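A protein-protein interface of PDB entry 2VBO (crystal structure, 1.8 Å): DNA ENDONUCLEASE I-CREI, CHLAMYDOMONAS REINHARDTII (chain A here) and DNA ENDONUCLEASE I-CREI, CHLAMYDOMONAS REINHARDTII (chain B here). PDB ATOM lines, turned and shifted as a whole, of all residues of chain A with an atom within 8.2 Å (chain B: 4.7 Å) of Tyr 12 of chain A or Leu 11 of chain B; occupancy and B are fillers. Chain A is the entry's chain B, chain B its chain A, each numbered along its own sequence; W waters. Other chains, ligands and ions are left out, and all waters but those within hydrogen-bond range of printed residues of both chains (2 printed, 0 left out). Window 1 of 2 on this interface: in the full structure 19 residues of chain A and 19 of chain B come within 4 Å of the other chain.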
ATOM      1  N   ASN A   6      -0.012  -4.056   0.217  1.00  0.00           N
ATOM      2  CA  ASN A   6       0.016  -4.954   1.354  1.00  0.00           C
ATOM      3  C   ASN A   6      -1.160  -5.952   1.337  1.00  0.00           C
ATOM      4  O   ASN A   6      -2.310  -5.573   1.080  1.00  0.00           O
ATOM      5  CB  ASN A   6       0.005  -4.040   2.581  1.00  0.00           C
ATOM      6  CG  ASN A   6      -0.424  -4.722   3.840  1.00  0.00           C
ATOM      7  OD1 ASN A   6      -1.601  -4.689   4.201  1.00  0.00           O
ATOM      8  ND2 ASN A   6       0.535  -5.296   4.559  1.00  0.00           N
ATOM      9  N   LYS A   7      -0.860  -7.216   1.625  1.00  0.00           N
ATOM     10  CA  LYS A   7      -1.827  -8.303   1.580  1.00  0.00           C
ATOM     11  C   LYS A   7      -3.034  -8.093   2.481  1.00  0.00           C
ATOM     12  O   LYS A   7      -4.156  -8.449   2.109  1.00  0.00           O
ATOM     13  CB  LYS A   7      -1.175  -9.632   1.962  1.00  0.00           C
ATOM     14  CG  LYS A   7      -2.083 -10.815   1.669  1.00  0.00           C
ATOM     15  CD  LYS A   7      -1.514 -12.133   2.162  1.00  0.00           C
ATOM     16  CE  LYS A   7      -2.414 -13.276   1.702  1.00  0.00           C
ATOM     17  NZ  LYS A   7      -1.690 -14.340   0.919  1.00  0.00           N
ATOM     18  N   GLU A   8      -2.800  -7.563   3.675  1.00  0.00           N
ATOM     19  CA  GLU A   8      -3.877  -7.351   4.636  1.00  0.00           C
ATOM     20  C   GLU A   8      -4.826  -6.275   4.117  1.00  0.00           C
ATOM     21  O   GLU A   8      -6.052  -6.351   4.303  1.00  0.00           O
ATOM     22  CB  GLU A   8      -3.311  -6.960   6.005  1.00  0.00           C
ATOM     23  CG  GLU A   8      -2.617  -8.164   6.677  1.00  0.00           C
ATOM     24  CD  GLU A   8      -2.116  -7.909   8.082  1.00  0.00           C
ATOM     25  OE1 GLU A   8      -2.425  -6.843   8.664  1.00  0.00           O
ATOM     26  OE2 GLU A   8      -1.393  -8.791   8.594  1.00  0.00           O
ATOM     27  N   PHE A   9      -4.273  -5.262   3.462  1.00  0.00           N
ATOM     28  CA  PHE A   9      -5.130  -4.263   2.818  1.00  0.00           C
ATOM     29  C   PHE A   9      -5.951  -4.873   1.672  1.00  0.00           C
ATOM     30  O   PHE A   9      -7.164  -4.636   1.540  1.00  0.00           O
ATOM     31  CB  PHE A   9      -4.252  -3.088   2.344  1.00  0.00           C
ATOM     32  CG  PHE A   9      -4.944  -2.127   1.424  1.00  0.00           C
ATOM     33  CD1 PHE A   9      -5.865  -1.231   1.910  1.00  0.00           C
ATOM     34  CD2 PHE A   9      -4.635  -2.105   0.068  1.00  0.00           C
ATOM     35  CE1 PHE A   9      -6.492  -0.327   1.048  1.00  0.00           C
ATOM     36  CE2 PHE A   9      -5.255  -1.212  -0.801  1.00  0.00           C
ATOM     37  CZ  PHE A   9      -6.186  -0.316  -0.302  1.00  0.00           C
ATOM     38  N   LEU A  10      -5.303  -5.664   0.825  1.00  0.00           N
ATOM     39  CA  LEU A  10      -6.036  -6.309  -0.262  1.00  0.00           C
ATOM     40  C   LEU A  10      -7.140  -7.249   0.228  1.00  0.00           C
ATOM     41  O   LEU A  10      -8.203  -7.334  -0.414  1.00  0.00           O
ATOM     42  CB  LEU A  10      -5.103  -7.049  -1.227  1.00  0.00           C
ATOM     43  CG  LEU A  10      -4.140  -6.121  -1.976  1.00  0.00           C
ATOM     44  CD1 LEU A  10      -3.038  -6.955  -2.616  1.00  0.00           C
ATOM     45  CD2 LEU A  10      -4.874  -5.258  -3.023  1.00  0.00           C
ATOM     46  N   LEU A  11      -6.879  -7.977   1.310  1.00  0.00           N
ATOM     47  CA  LEU A  11      -7.884  -8.892   1.837  1.00  0.00           C
ATOM     48  C   LEU A  11      -9.115  -8.118   2.282  1.00  0.00           C
ATOM     49  O   LEU A  11     -10.211  -8.430   1.891  1.00  0.00           O
ATOM     50  CB  LEU A  11      -7.363  -9.740   2.983  1.00  0.00           C
ATOM     51  CG  LEU A  11      -6.560 -10.980   2.557  1.00  0.00           C
ATOM     52  CD1 LEU A  11      -5.706 -11.370   3.753  1.00  0.00           C
ATOM     53  CD2 LEU A  11      -7.565 -12.126   2.198  1.00  0.00           C
ATOM     54  N   TYR A  12      -8.907  -7.096   3.087  1.00  0.00           N
ATOM     55  CA  TYR A  12     -10.004  -6.271   3.573  1.00  0.00           C
ATOM     56  C   TYR A  12     -10.719  -5.603   2.388  1.00  0.00           C
ATOM     57  O   TYR A  12     -11.957  -5.582   2.309  1.00  0.00           O
ATOM     58  CB  TYR A  12      -9.428  -5.191   4.487  1.00  0.00           C
ATOM     59  CG  TYR A  12     -10.518  -4.197   4.859  1.00  0.00           C
ATOM     60  CD1 TYR A  12     -11.329  -4.410   5.973  1.00  0.00           C
ATOM     61  CD2 TYR A  12     -10.801  -3.100   4.027  1.00  0.00           C
ATOM     62  CE1 TYR A  12     -12.379  -3.478   6.305  1.00  0.00           C
ATOM     63  CE2 TYR A  12     -11.851  -2.202   4.307  1.00  0.00           C
ATOM     64  CZ  TYR A  12     -12.641  -2.390   5.447  1.00  0.00           C
ATOM     65  OH  TYR A  12     -13.670  -1.486   5.707  1.00  0.00           O
ATOM     66  N   LEU A  13      -9.946  -5.016   1.473  1.00  0.00           N
ATOM     67  CA  LEU A  13     -10.547  -4.289   0.366  1.00  0.00           C
ATOM     68  C   LEU A  13     -11.370  -5.230  -0.526  1.00  0.00           C
ATOM     69  O   LEU A  13     -12.430  -4.875  -1.043  1.00  0.00           O
ATOM     70  CB  LEU A  13      -9.472  -3.556  -0.451  1.00  0.00           C
ATOM     71  CG  LEU A  13      -9.982  -2.656  -1.588  1.00  0.00           C
ATOM     72  CD1 LEU A  13     -10.943  -1.591  -1.036  1.00  0.00           C
ATOM     73  CD2 LEU A  13      -8.747  -1.980  -2.316  1.00  0.00           C
ATOM     74  N   ALA A  14     -10.876  -6.436  -0.739  1.00  0.00           N
ATOM     75  CA  ALA A  14     -11.627  -7.385  -1.559  1.00  0.00           C
ATOM     76  C   ALA A  14     -13.023  -7.630  -0.960  1.00  0.00           C
ATOM     77  O   ALA A  14     -14.029  -7.659  -1.692  1.00  0.00           O
ATOM     78  CB  ALA A  14     -10.854  -8.697  -1.687  1.00  0.00           C
ATOM     79  N   GLY A  15     -13.088  -7.772   0.363  1.00  0.00           N
ATOM     80  CA  GLY A  15     -14.368  -7.980   1.042  1.00  0.00           C
ATOM     81  C   GLY A  15     -15.238  -6.742   0.870  1.00  0.00           C
ATOM     82  O   GLY A  15     -16.431  -6.847   0.544  1.00  0.00           O
ATOM     83  N   PHE A  16     -14.662  -5.562   1.076  1.00  0.00           N
ATOM     84  CA  PHE A  16     -15.437  -4.325   0.907  1.00  0.00           C
ATOM     85  C   PHE A  16     -15.971  -4.127  -0.510  1.00  0.00           C
ATOM     86  O   PHE A  16     -17.104  -3.698  -0.722  1.00  0.00           O
ATOM     87  CB  PHE A  16     -14.605  -3.093   1.290  1.00  0.00           C
ATOM     88  CG  PHE A  16     -15.464  -1.870   1.540  1.00  0.00           C
ATOM     89  CD1 PHE A  16     -16.231  -1.794   2.686  1.00  0.00           C
ATOM     90  CD2 PHE A  16     -15.601  -0.873   0.600  1.00  0.00           C
ATOM     91  CE1 PHE A  16     -17.062  -0.703   2.935  1.00  0.00           C
ATOM     92  CE2 PHE A  16     -16.440   0.233   0.844  1.00  0.00           C
ATOM     93  CZ  PHE A  16     -17.172   0.307   1.990  1.00  0.00           C
ATOM     94  N   VAL A  17     -15.130  -4.432  -1.489  1.00  0.00           N
ATOM     95  CA  VAL A  17     -15.530  -4.337  -2.883  1.00  0.00           C
ATOM     96  C   VAL A  17     -16.591  -5.389  -3.202  1.00  0.00           C
ATOM     97  O   VAL A  17     -17.565  -5.088  -3.885  1.00  0.00           O
ATOM     98  CB  VAL A  17     -14.319  -4.525  -3.786  1.00  0.00           C
ATOM     99  CG1 VAL A  17     -14.750  -4.833  -5.215  1.00  0.00           C
ATOM    100  CG2 VAL A  17     -13.411  -3.297  -3.673  1.00  0.00           C
ATOM    101  N   ASP A  18     -16.430  -6.614  -2.710  1.00  0.00           N
ATOM    102  CA  ASP A  18     -17.479  -7.605  -2.939  1.00  0.00           C
ATOM    103  C   ASP A  18     -18.795  -7.108  -2.324  1.00  0.00           C
ATOM    104  O   ASP A  18     -19.858  -7.464  -2.809  1.00  0.00           O
ATOM    105  CB  ASP A  18     -17.112  -8.982  -2.366  1.00  0.00           C
ATOM    106  CG  ASP A  18     -16.299  -9.845  -3.337  1.00  0.00           C
ATOM    107  OD1 ASP A  18     -16.277  -9.575  -4.575  1.00  0.00           O
ATOM    108  OD2 ASP A  18     -15.694 -10.813  -2.832  1.00  0.00           O
ATOM    109  N   GLY A  19     -18.742  -6.286  -1.272  1.00  0.00           N
ATOM    110  CA  GLY A  19     -19.967  -5.700  -0.708  1.00  0.00           C
ATOM    111  C   GLY A  19     -20.493  -4.490  -1.499  1.00  0.00           C
ATOM    112  O   GLY A  19     -21.533  -4.583  -2.162  1.00  0.00           O
ATOM    113  N   TRP A  53     -15.321  10.253   3.543  1.00  0.00           N
ATOM    114  CA  TRP A  53     -13.970  10.221   4.097  1.00  0.00           C
ATOM    115  C   TRP A  53     -13.314   8.873   3.830  1.00  0.00           C
ATOM    116  O   TRP A  53     -12.111   8.795   3.606  1.00  0.00           O
ATOM    117  CB  TRP A  53     -13.952  10.539   5.604  1.00  0.00           C
ATOM    118  CG  TRP A  53     -14.648   9.535   6.473  1.00  0.00           C
ATOM    119  CD1 TRP A  53     -15.957   9.563   6.876  1.00  0.00           C
ATOM    120  CD2 TRP A  53     -14.082   8.344   7.018  1.00  0.00           C
ATOM    121  NE1 TRP A  53     -16.234   8.466   7.666  1.00  0.00           N
ATOM    122  CE2 TRP A  53     -15.093   7.716   7.787  1.00  0.00           C
ATOM    123  CE3 TRP A  53     -12.795   7.774   6.993  1.00  0.00           C
ATOM    124  CZ2 TRP A  53     -14.878   6.516   8.461  1.00  0.00           C
ATOM    125  CZ3 TRP A  53     -12.579   6.600   7.680  1.00  0.00           C
ATOM    126  CH2 TRP A  53     -13.615   5.973   8.400  1.00  0.00           C
ATOM    127  N   PHE A  54     -14.119   7.817   3.842  1.00  0.00           N
ATOM    128  CA  PHE A  54     -13.593   6.472   3.624  1.00  0.00           C
ATOM    129  C   PHE A  54     -13.103   6.313   2.182  1.00  0.00           C
ATOM    130  O   PHE A  54     -12.067   5.672   1.930  1.00  0.00           O
ATOM    131  CB  PHE A  54     -14.695   5.456   3.916  1.00  0.00           C
ATOM    132  CG  PHE A  54     -14.215   4.038   4.016  1.00  0.00           C
ATOM    133  CD1 PHE A  54     -14.530   3.103   3.034  1.00  0.00           C
ATOM    134  CD2 PHE A  54     -13.459   3.631   5.100  1.00  0.00           C
ATOM    135  CE1 PHE A  54     -14.094   1.775   3.154  1.00  0.00           C
ATOM    136  CE2 PHE A  54     -13.050   2.319   5.210  1.00  0.00           C
ATOM    137  CZ  PHE A  54     -13.372   1.397   4.247  1.00  0.00           C
ATOM    138  N   LEU A  58      -9.373   5.795   0.550  1.00  0.00           N
ATOM    139  CA  LEU A  58      -9.159   4.822  -0.516  1.00  0.00           C
ATOM    140  C   LEU A  58      -8.338   5.399  -1.672  1.00  0.00           C
ATOM    141  O   LEU A  58      -7.419   4.745  -2.202  1.00  0.00           O
ATOM    142  CB  LEU A  58     -10.519   4.396  -1.056  1.00  0.00           C
ATOM    143  CG  LEU A  58     -10.725   2.957  -1.502  1.00  0.00           C
ATOM    144  CD1 LEU A  58     -10.160   2.022  -0.422  1.00  0.00           C
ATOM    145  CD2 LEU A  58     -12.206   2.727  -1.711  1.00  0.00           C
ATOM    146  N   GLU A  61      -4.770   5.385  -0.487  1.00  0.00           N
ATOM    147  CA  GLU A  61      -4.257   4.033  -0.272  1.00  0.00           C
ATOM    148  C   GLU A  61      -4.050   3.292  -1.590  1.00  0.00           C
ATOM    149  O   GLU A  61      -3.040   2.609  -1.775  1.00  0.00           O
ATOM    150  CB  GLU A  61      -5.196   3.265   0.670  1.00  0.00           C
ATOM    151  CG  GLU A  61      -5.102   3.756   2.140  1.00  0.00           C
ATOM    152  CD  GLU A  61      -6.284   3.304   3.015  1.00  0.00           C
ATOM    153  OE1 GLU A  61      -7.259   2.713   2.499  1.00  0.00           O
ATOM    154  OE2 GLU A  61      -6.239   3.543   4.240  1.00  0.00           O
ATOM    155  N   LEU A  91      -5.845  -7.161  -6.767  1.00  0.00           N
ATOM    156  CA  LEU A  91      -7.071  -7.419  -6.030  1.00  0.00           C
ATOM    157  C   LEU A  91      -7.670  -8.798  -6.317  1.00  0.00           C
ATOM    158  O   LEU A  91      -8.146  -9.463  -5.413  1.00  0.00           O
ATOM    159  CB  LEU A  91      -8.107  -6.336  -6.329  1.00  0.00           C
ATOM    160  CG  LEU A  91      -9.289  -6.343  -5.351  1.00  0.00           C
ATOM    161  CD1 LEU A  91      -8.819  -5.960  -3.935  1.00  0.00           C
ATOM    162  CD2 LEU A  91     -10.349  -5.335  -5.864  1.00  0.00           C
ATOM    163  N   PHE A  94      -8.245 -12.176  -4.311  1.00  0.00           N
ATOM    164  CA  PHE A  94      -8.875 -12.126  -2.998  1.00  0.00           C
ATOM    165  C   PHE A  94     -10.398 -11.953  -3.080  1.00  0.00           C
ATOM    166  O   PHE A  94     -11.084 -12.022  -2.063  1.00  0.00           O
ATOM    167  CB  PHE A  94      -8.230 -11.012  -2.160  1.00  0.00           C
ATOM    168  CG  PHE A  94      -6.768 -11.221  -1.934  1.00  0.00           C
ATOM    169  CD1 PHE A  94      -6.327 -12.288  -1.162  1.00  0.00           C
ATOM    170  CD2 PHE A  94      -5.820 -10.400  -2.539  1.00  0.00           C
ATOM    171  CE1 PHE A  94      -4.951 -12.525  -0.970  1.00  0.00           C
ATOM    172  CE2 PHE A  94      -4.449 -10.632  -2.355  1.00  0.00           C
ATOM    173  CZ  PHE A  94      -4.017 -11.689  -1.568  1.00  0.00           C
ATOM    174  N   LEU A  95     -10.909 -11.687  -4.285  1.00  0.00           N
ATOM    175  CA  LEU A  95     -12.339 -11.517  -4.525  1.00  0.00           C
ATOM    176  C   LEU A  95     -13.067 -12.869  -4.532  1.00  0.00           C
ATOM    177  O   LEU A  95     -12.483 -13.887  -4.948  1.00  0.00           O
ATOM    178  CB  LEU A  95     -12.565 -10.780  -5.859  1.00  0.00           C
ATOM    179  CG  LEU A  95     -12.123  -9.308  -5.959  1.00  0.00           C
ATOM    180  CD1 LEU A  95     -12.235  -8.813  -7.397  1.00  0.00           C
ATOM    181  CD2 LEU A  95     -12.906  -8.390  -5.037  1.00  0.00           C
ATOM    182  N   LYS A  96     -14.311 -12.876  -4.050  1.00  0.00           N
ATOM    183  CA  LYS A  96     -15.164 -14.071  -4.029  1.00  0.00           C
ATOM    184  C   LYS A  96     -16.466 -13.925  -4.835  1.00  0.00           C
ATOM    185  O   LYS A  96     -16.977 -14.916  -5.400  1.00  0.00           O
ATOM    186  CB  LYS A  96     -15.564 -14.421  -2.588  1.00  0.00           C
ATOM    187  CG  LYS A  96     -14.385 -14.616  -1.638  1.00  0.00           C
ATOM    188  CD  LYS A  96     -14.866 -14.963  -0.250  1.00  0.00           C
ATOM    189  CE  LYS A  96     -13.669 -15.391   0.608  1.00  0.00           C
ATOM    190  NZ  LYS A  96     -14.084 -15.494   2.036  1.00  0.00           N
ATOM    191  N   LYS B   7      -7.135 -15.569  10.418  1.00  0.00           N
ATOM    192  CA  LYS B   7      -6.811 -14.168  10.149  1.00  0.00           C
ATOM    193  C   LYS B   7      -7.326 -13.716   8.782  1.00  0.00           C
ATOM    194  O   LYS B   7      -7.950 -12.655   8.643  1.00  0.00           O
ATOM    195  CB  LYS B   7      -5.279 -13.980  10.209  1.00  0.00           C
ATOM    196  CG  LYS B   7      -4.790 -12.647   9.638  1.00  0.00           C
ATOM    197  CD  LYS B   7      -3.344 -12.374  10.068  1.00  0.00           C
ATOM    198  CE  LYS B   7      -2.946 -10.971   9.658  1.00  0.00           C
ATOM    199  NZ  LYS B   7      -1.469 -10.794   9.565  1.00  0.00           N
ATOM    200  N   GLU B   8      -7.041 -14.498   7.745  1.00  0.00           N
ATOM    201  CA  GLU B   8      -7.372 -14.026   6.411  1.00  0.00           C
ATOM    202  C   GLU B   8      -8.899 -14.028   6.256  1.00  0.00           C
ATOM    203  O   GLU B   8      -9.449 -13.194   5.546  1.00  0.00           O
ATOM    204  CB  GLU B   8      -6.688 -14.885   5.348  1.00  0.00           C
ATOM    205  CG  GLU B   8      -5.157 -14.782   5.379  1.00  0.00           C
ATOM    206  CD  GLU B   8      -4.500 -15.647   4.322  1.00  0.00           C
ATOM    207  OE1 GLU B   8      -5.203 -16.464   3.665  1.00  0.00           O
ATOM    208  OE2 GLU B   8      -3.266 -15.491   4.168  1.00  0.00           O
ATOM    209  N   PHE B   9      -9.597 -14.961   6.910  1.00  0.00           N
ATOM    210  CA  PHE B   9     -11.066 -14.974   6.843  1.00  0.00           C
ATOM    211  C   PHE B   9     -11.627 -13.739   7.541  1.00  0.00           C
ATOM    212  O   PHE B   9     -12.501 -13.055   6.988  1.00  0.00           O
ATOM    213  CB  PHE B   9     -11.577 -16.224   7.564  1.00  0.00           C
ATOM    214  CG  PHE B   9     -13.008 -16.158   8.024  1.00  0.00           C
ATOM    215  CD1 PHE B   9     -14.050 -16.225   7.113  1.00  0.00           C
ATOM    216  CD2 PHE B   9     -13.312 -16.119   9.386  1.00  0.00           C
ATOM    217  CE1 PHE B   9     -15.376 -16.239   7.541  1.00  0.00           C
ATOM    218  CE2 PHE B   9     -14.627 -16.117   9.816  1.00  0.00           C
ATOM    219  CZ  PHE B   9     -15.655 -16.194   8.885  1.00  0.00           C
ATOM    220  N   LEU B  10     -11.112 -13.437   8.733  1.00  0.00           N
ATOM    221  CA  LEU B  10     -11.556 -12.222   9.468  1.00  0.00           C
ATOM    222  C   LEU B  10     -11.272 -10.934   8.720  1.00  0.00           C
ATOM    223  O   LEU B  10     -12.086 -10.019   8.754  1.00  0.00           O
ATOM    224  CB  LEU B  10     -10.943 -12.121  10.868  1.00  0.00           C
ATOM    225  CG  LEU B  10     -11.297 -13.281  11.796  1.00  0.00           C
ATOM    226  CD1 LEU B  10     -10.293 -13.290  12.975  1.00  0.00           C
ATOM    227  CD2 LEU B  10     -12.751 -13.098  12.308  1.00  0.00           C
ATOM    228  N   LEU B  11     -10.110 -10.833   8.080  1.00  0.00           N
ATOM    229  CA  LEU B  11      -9.798  -9.627   7.274  1.00  0.00           C
ATOM    230  C   LEU B  11     -10.794  -9.445   6.123  1.00  0.00           C
ATOM    231  O   LEU B  11     -11.353  -8.358   5.946  1.00  0.00           O
ATOM    232  CB  LEU B  11      -8.361  -9.688   6.719  1.00  0.00           C
ATOM    233  CG  LEU B  11      -7.271  -9.226   7.699  1.00  0.00           C
ATOM    234  CD1 LEU B  11      -5.947  -9.753   7.172  1.00  0.00           C
ATOM    235  CD2 LEU B  11      -7.281  -7.689   7.689  1.00  0.00           C
ATOM    236  N   TYR B  12     -11.024 -10.499   5.337  1.00  0.00           N
ATOM    237  CA  TYR B  12     -11.964 -10.391   4.215  1.00  0.00           C
ATOM    238  C   TYR B  12     -13.369 -10.118   4.756  1.00  0.00           C
ATOM    239  O   TYR B  12     -14.083  -9.218   4.281  1.00  0.00           O
ATOM    240  CB  TYR B  12     -11.948 -11.672   3.371  1.00  0.00           C
ATOM    241  CG  TYR B  12     -13.057 -11.695   2.346  1.00  0.00           C
ATOM    242  CD1 TYR B  12     -12.820 -11.261   1.043  1.00  0.00           C
ATOM    243  CD2 TYR B  12     -14.356 -12.096   2.703  1.00  0.00           C
ATOM    244  CE1 TYR B  12     -13.842 -11.209   0.105  1.00  0.00           C
ATOM    245  CE2 TYR B  12     -15.399 -12.077   1.757  1.00  0.00           C
ATOM    246  CZ  TYR B  12     -15.131 -11.637   0.466  1.00  0.00           C
ATOM    247  OH  TYR B  12     -16.166 -11.626  -0.430  1.00  0.00           O
ATOM    248  N   LEU B  13     -13.770 -10.867   5.776  1.00  0.00           N
ATOM    249  CA  LEU B  13     -15.127 -10.713   6.304  1.00  0.00           C
ATOM    250  C   LEU B  13     -15.348  -9.331   6.885  1.00  0.00           C
ATOM    251  O   LEU B  13     -16.434  -8.773   6.706  1.00  0.00           O
ATOM    252  CB  LEU B  13     -15.480 -11.802   7.317  1.00  0.00           C
ATOM    253  CG  LEU B  13     -16.954 -11.815   7.766  1.00  0.00           C
ATOM    254  CD1 LEU B  13     -17.949 -11.896   6.587  1.00  0.00           C
ATOM    255  CD2 LEU B  13     -17.115 -13.053   8.669  1.00  0.00           C
ATOM    256  N   ALA B  14     -14.318  -8.753   7.517  1.00  0.00           N
ATOM    257  CA  ALA B  14     -14.467  -7.401   8.091  1.00  0.00           C
ATOM    258  C   ALA B  14     -14.815  -6.409   6.971  1.00  0.00           C
ATOM    259  O   ALA B  14     -15.689  -5.549   7.124  1.00  0.00           O
ATOM    260  CB  ALA B  14     -13.183  -6.980   8.814  1.00  0.00           C
ATOM    261  N   GLY B  15     -14.141  -6.543   5.832  1.00  0.00           N
ATOM    262  CA  GLY B  15     -14.423  -5.696   4.653  1.00  0.00           C
ATOM    263  C   GLY B  15     -15.851  -5.909   4.192  1.00  0.00           C
ATOM    264  O   GLY B  15     -16.584  -4.931   3.939  1.00  0.00           O
ATOM    265  N   ASP B  18     -18.324  -4.415   6.651  1.00  0.00           N
ATOM    266  CA  ASP B  18     -18.360  -2.953   6.517  1.00  0.00           C
ATOM    267  C   ASP B  18     -19.165  -2.591   5.278  1.00  0.00           C
ATOM    268  O   ASP B  18     -19.829  -1.549   5.260  1.00  0.00           O
ATOM    269  CB  ASP B  18     -16.953  -2.350   6.437  1.00  0.00           C
ATOM    270  CG  ASP B  18     -16.330  -2.113   7.813  1.00  0.00           C
ATOM    271  OD1 ASP B  18     -17.066  -2.104   8.845  1.00  0.00           O
ATOM    272  OD2 ASP B  18     -15.093  -1.918   7.842  1.00  0.00           O
ATOM    273  N   PHE B  94     -10.436  -5.579  12.755  1.00  0.00           N
ATOM    274  CA  PHE B  94     -10.269  -5.389  11.319  1.00  0.00           C
ATOM    275  C   PHE B  94     -11.354  -4.517  10.688  1.00  0.00           C
ATOM    276  O   PHE B  94     -11.232  -4.131   9.512  1.00  0.00           O
ATOM    277  CB  PHE B  94     -10.222  -6.739  10.621  1.00  0.00           C
ATOM    278  CG  PHE B  94      -9.116  -7.633  11.137  1.00  0.00           C
ATOM    279  CD1 PHE B  94      -7.787  -7.296  10.958  1.00  0.00           C
ATOM    280  CD2 PHE B  94      -9.415  -8.788  11.824  1.00  0.00           C
ATOM    281  CE1 PHE B  94      -6.759  -8.108  11.447  1.00  0.00           C
ATOM    282  CE2 PHE B  94      -8.404  -9.625  12.279  1.00  0.00           C
ATOM    283  CZ  PHE B  94      -7.070  -9.276  12.105  1.00  0.00           C
ATOM    284  N   LYS B  96     -13.552  -1.137   9.978  1.00  0.00           N
ATOM    285  CA  LYS B  96     -13.201   0.279   9.768  1.00  0.00           C
ATOM    286  C   LYS B  96     -14.431   1.186   9.852  1.00  0.00           C
ATOM    287  O   LYS B  96     -14.332   2.356  10.251  1.00  0.00           O
ATOM    288  CB  LYS B  96     -12.544   0.477   8.409  1.00  0.00           C
ATOM    289  CG  LYS B  96     -11.195  -0.236   8.306  1.00  0.00           C
ATOM    290  CD  LYS B  96     -10.487   0.099   7.018  1.00  0.00           C
ATOM    291  CE  LYS B  96      -9.244  -0.774   6.871  1.00  0.00           C
ATOM    292  NZ  LYS B  96      -8.434  -0.359   5.682  1.00  0.00           N
HETATM  293  O   HOH W   1      -7.378   1.967   7.113  1.00  0.00           O
HETATM  294  O   HOH W   2      -3.738 -16.052   0.873  1.00  0.00           O
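The side-chain carboxylate (OE2) of Glu 8 of chain B lies within salt-bridge range of the side-chain amino group (NZ) of Lys 7 of chain A. The side-chain hydroxyl of Tyr 12 of chain B is in hydrogen-bond range of the side-chain carboxylate of Asp 18 of chain A (2.6 Å). OD2 of Asp 18 of chain B sits at hydrogen-bond distance from OH of Tyr 12 of chain A, at 2.6 Å. The side-chain amino group (NZ) of Lys 7 of chain B lies close to the side-chain carboxylate (OE2) of Glu 8 of chain A, 2.2 Å away.
The backbone NH (N) of Lys 96 of chain B lies within hydrogen-bond range of the side-chain carboxylate (OD2) of Asp 18 of chain B, at 2.7 Å. The side-chain amide oxygen (OD1) of Asn 6 of chain A lies within hydrogen-bond range of the backbone NH (N) of Glu 8 of chain A (3.2 Å). The side-chain carboxylate of Asp 18 of chain A sits at hydrogen-bond distance from the backbone NH of Lys 96 of chain A (2.8 Å).
Among the printed residues, pairs that only touch across the chains: Phe 16 of chain A with Gly 15 of chain B (3.3 Å), Gly 15 of chain A with Tyr 12 of chain B (3.4 Å), Tyr 12 of chain A with Gly 15 of chain B (3.4 Å), Lys 96 of chain A with Tyr 12 of chain B (3.4 Å), Tyr 12 of chain A with Leu 11 of chain B (3.4 Å), Tyr 12 of chain A with Phe 94 of chain B (3.5 Å), Gly 15 of chain A with Gly 15 of chain B (3.5 Å), Leu 11 of chain A with Tyr 12 of chain B (3.5 Å), Tyr 12 of chain A with Lys 96 of chain B (3.5 Å), Phe 94 of chain A with Tyr 12 of chain B (3.6 Å), Phe 16 of chain A with Asp 18 of chain B (3.7 Å), Glu 8 of chain A with Leu 11 of chain B (3.7 Å), Phe 54 of chain A with Lys 96 of chain B (3.7 Å), Leu 11 of chain A with Leu 11 of chain B (3.8 Å), Leu 11 of chain A with Glu 8 of chain B (3.8 Å), Ala 14 of chain A with Tyr 12 of chain B (3.8 Å) and Tyr 12 of chain A with Ala 14 of chain B (3.9 Å).
Of chain B, only Leu 11 (3.4 Å), Ala 14 (3.9 Å), Gly 15 (3.4 Å), Asp 18 (2.6 Å), Phe 94 (3.5 Å) and Lys 96 (3.5 Å) come within 4 Å of Tyr 12 of chain A. Leu 11 of chain B touches just these residues of chain A: Glu 8 (3.7 Å), Leu 11 (3.8 Å) and Tyr 12 (3.4 Å). Ala 14 of chain B touches one residue of chain A. Of the printed residues of chain B, Leu 11 of chain A touches Glu 8, Leu 11 and Tyr 12. Of the printed residues of chain A, Asp 18 of chain B touches Tyr 12 (2.6 Å) and Phe 16 (3.7 Å). Of the printed residues of chain A, Lys 7 of chain B touches Glu 8 (2.2 Å). The nearest residue of chain B that does not touch Tyr 12 of chain A is Tyr 12 of chain B (4.6 Å). The nearest residue of chain A that does not touch Leu 11 of chain B is Lys 7 of chain A (5.5 Å).
Of the 22 printed residues of chain A, 11 touch a printed residue of chain B. Of the 12 printed residues of chain B, 9 touch a printed residue of chain A. Among the printed residues, 21 pairs touch across the chains. Among the printed residues, Asp or Glu carboxylates within 4 Å of a Lys or Arg side-chain nitrogen of the other chain: Lys 7 of chain A with Glu 8 of chain B and Glu 8 of chain A with Lys 7 of chain B.
Water W2 lies within hydrogen-bond range of the side-chain amino group of Lys 7 of chain A (2.7 Å) and the side-chain carboxylate of Glu 8 of chain B (3.2 Å). Water W1 bridges the side-chain amino group of Lys 96 of chain B (2.9 Å) and the side-chain carboxylate of Glu 61 of chain A (3.5 Å).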
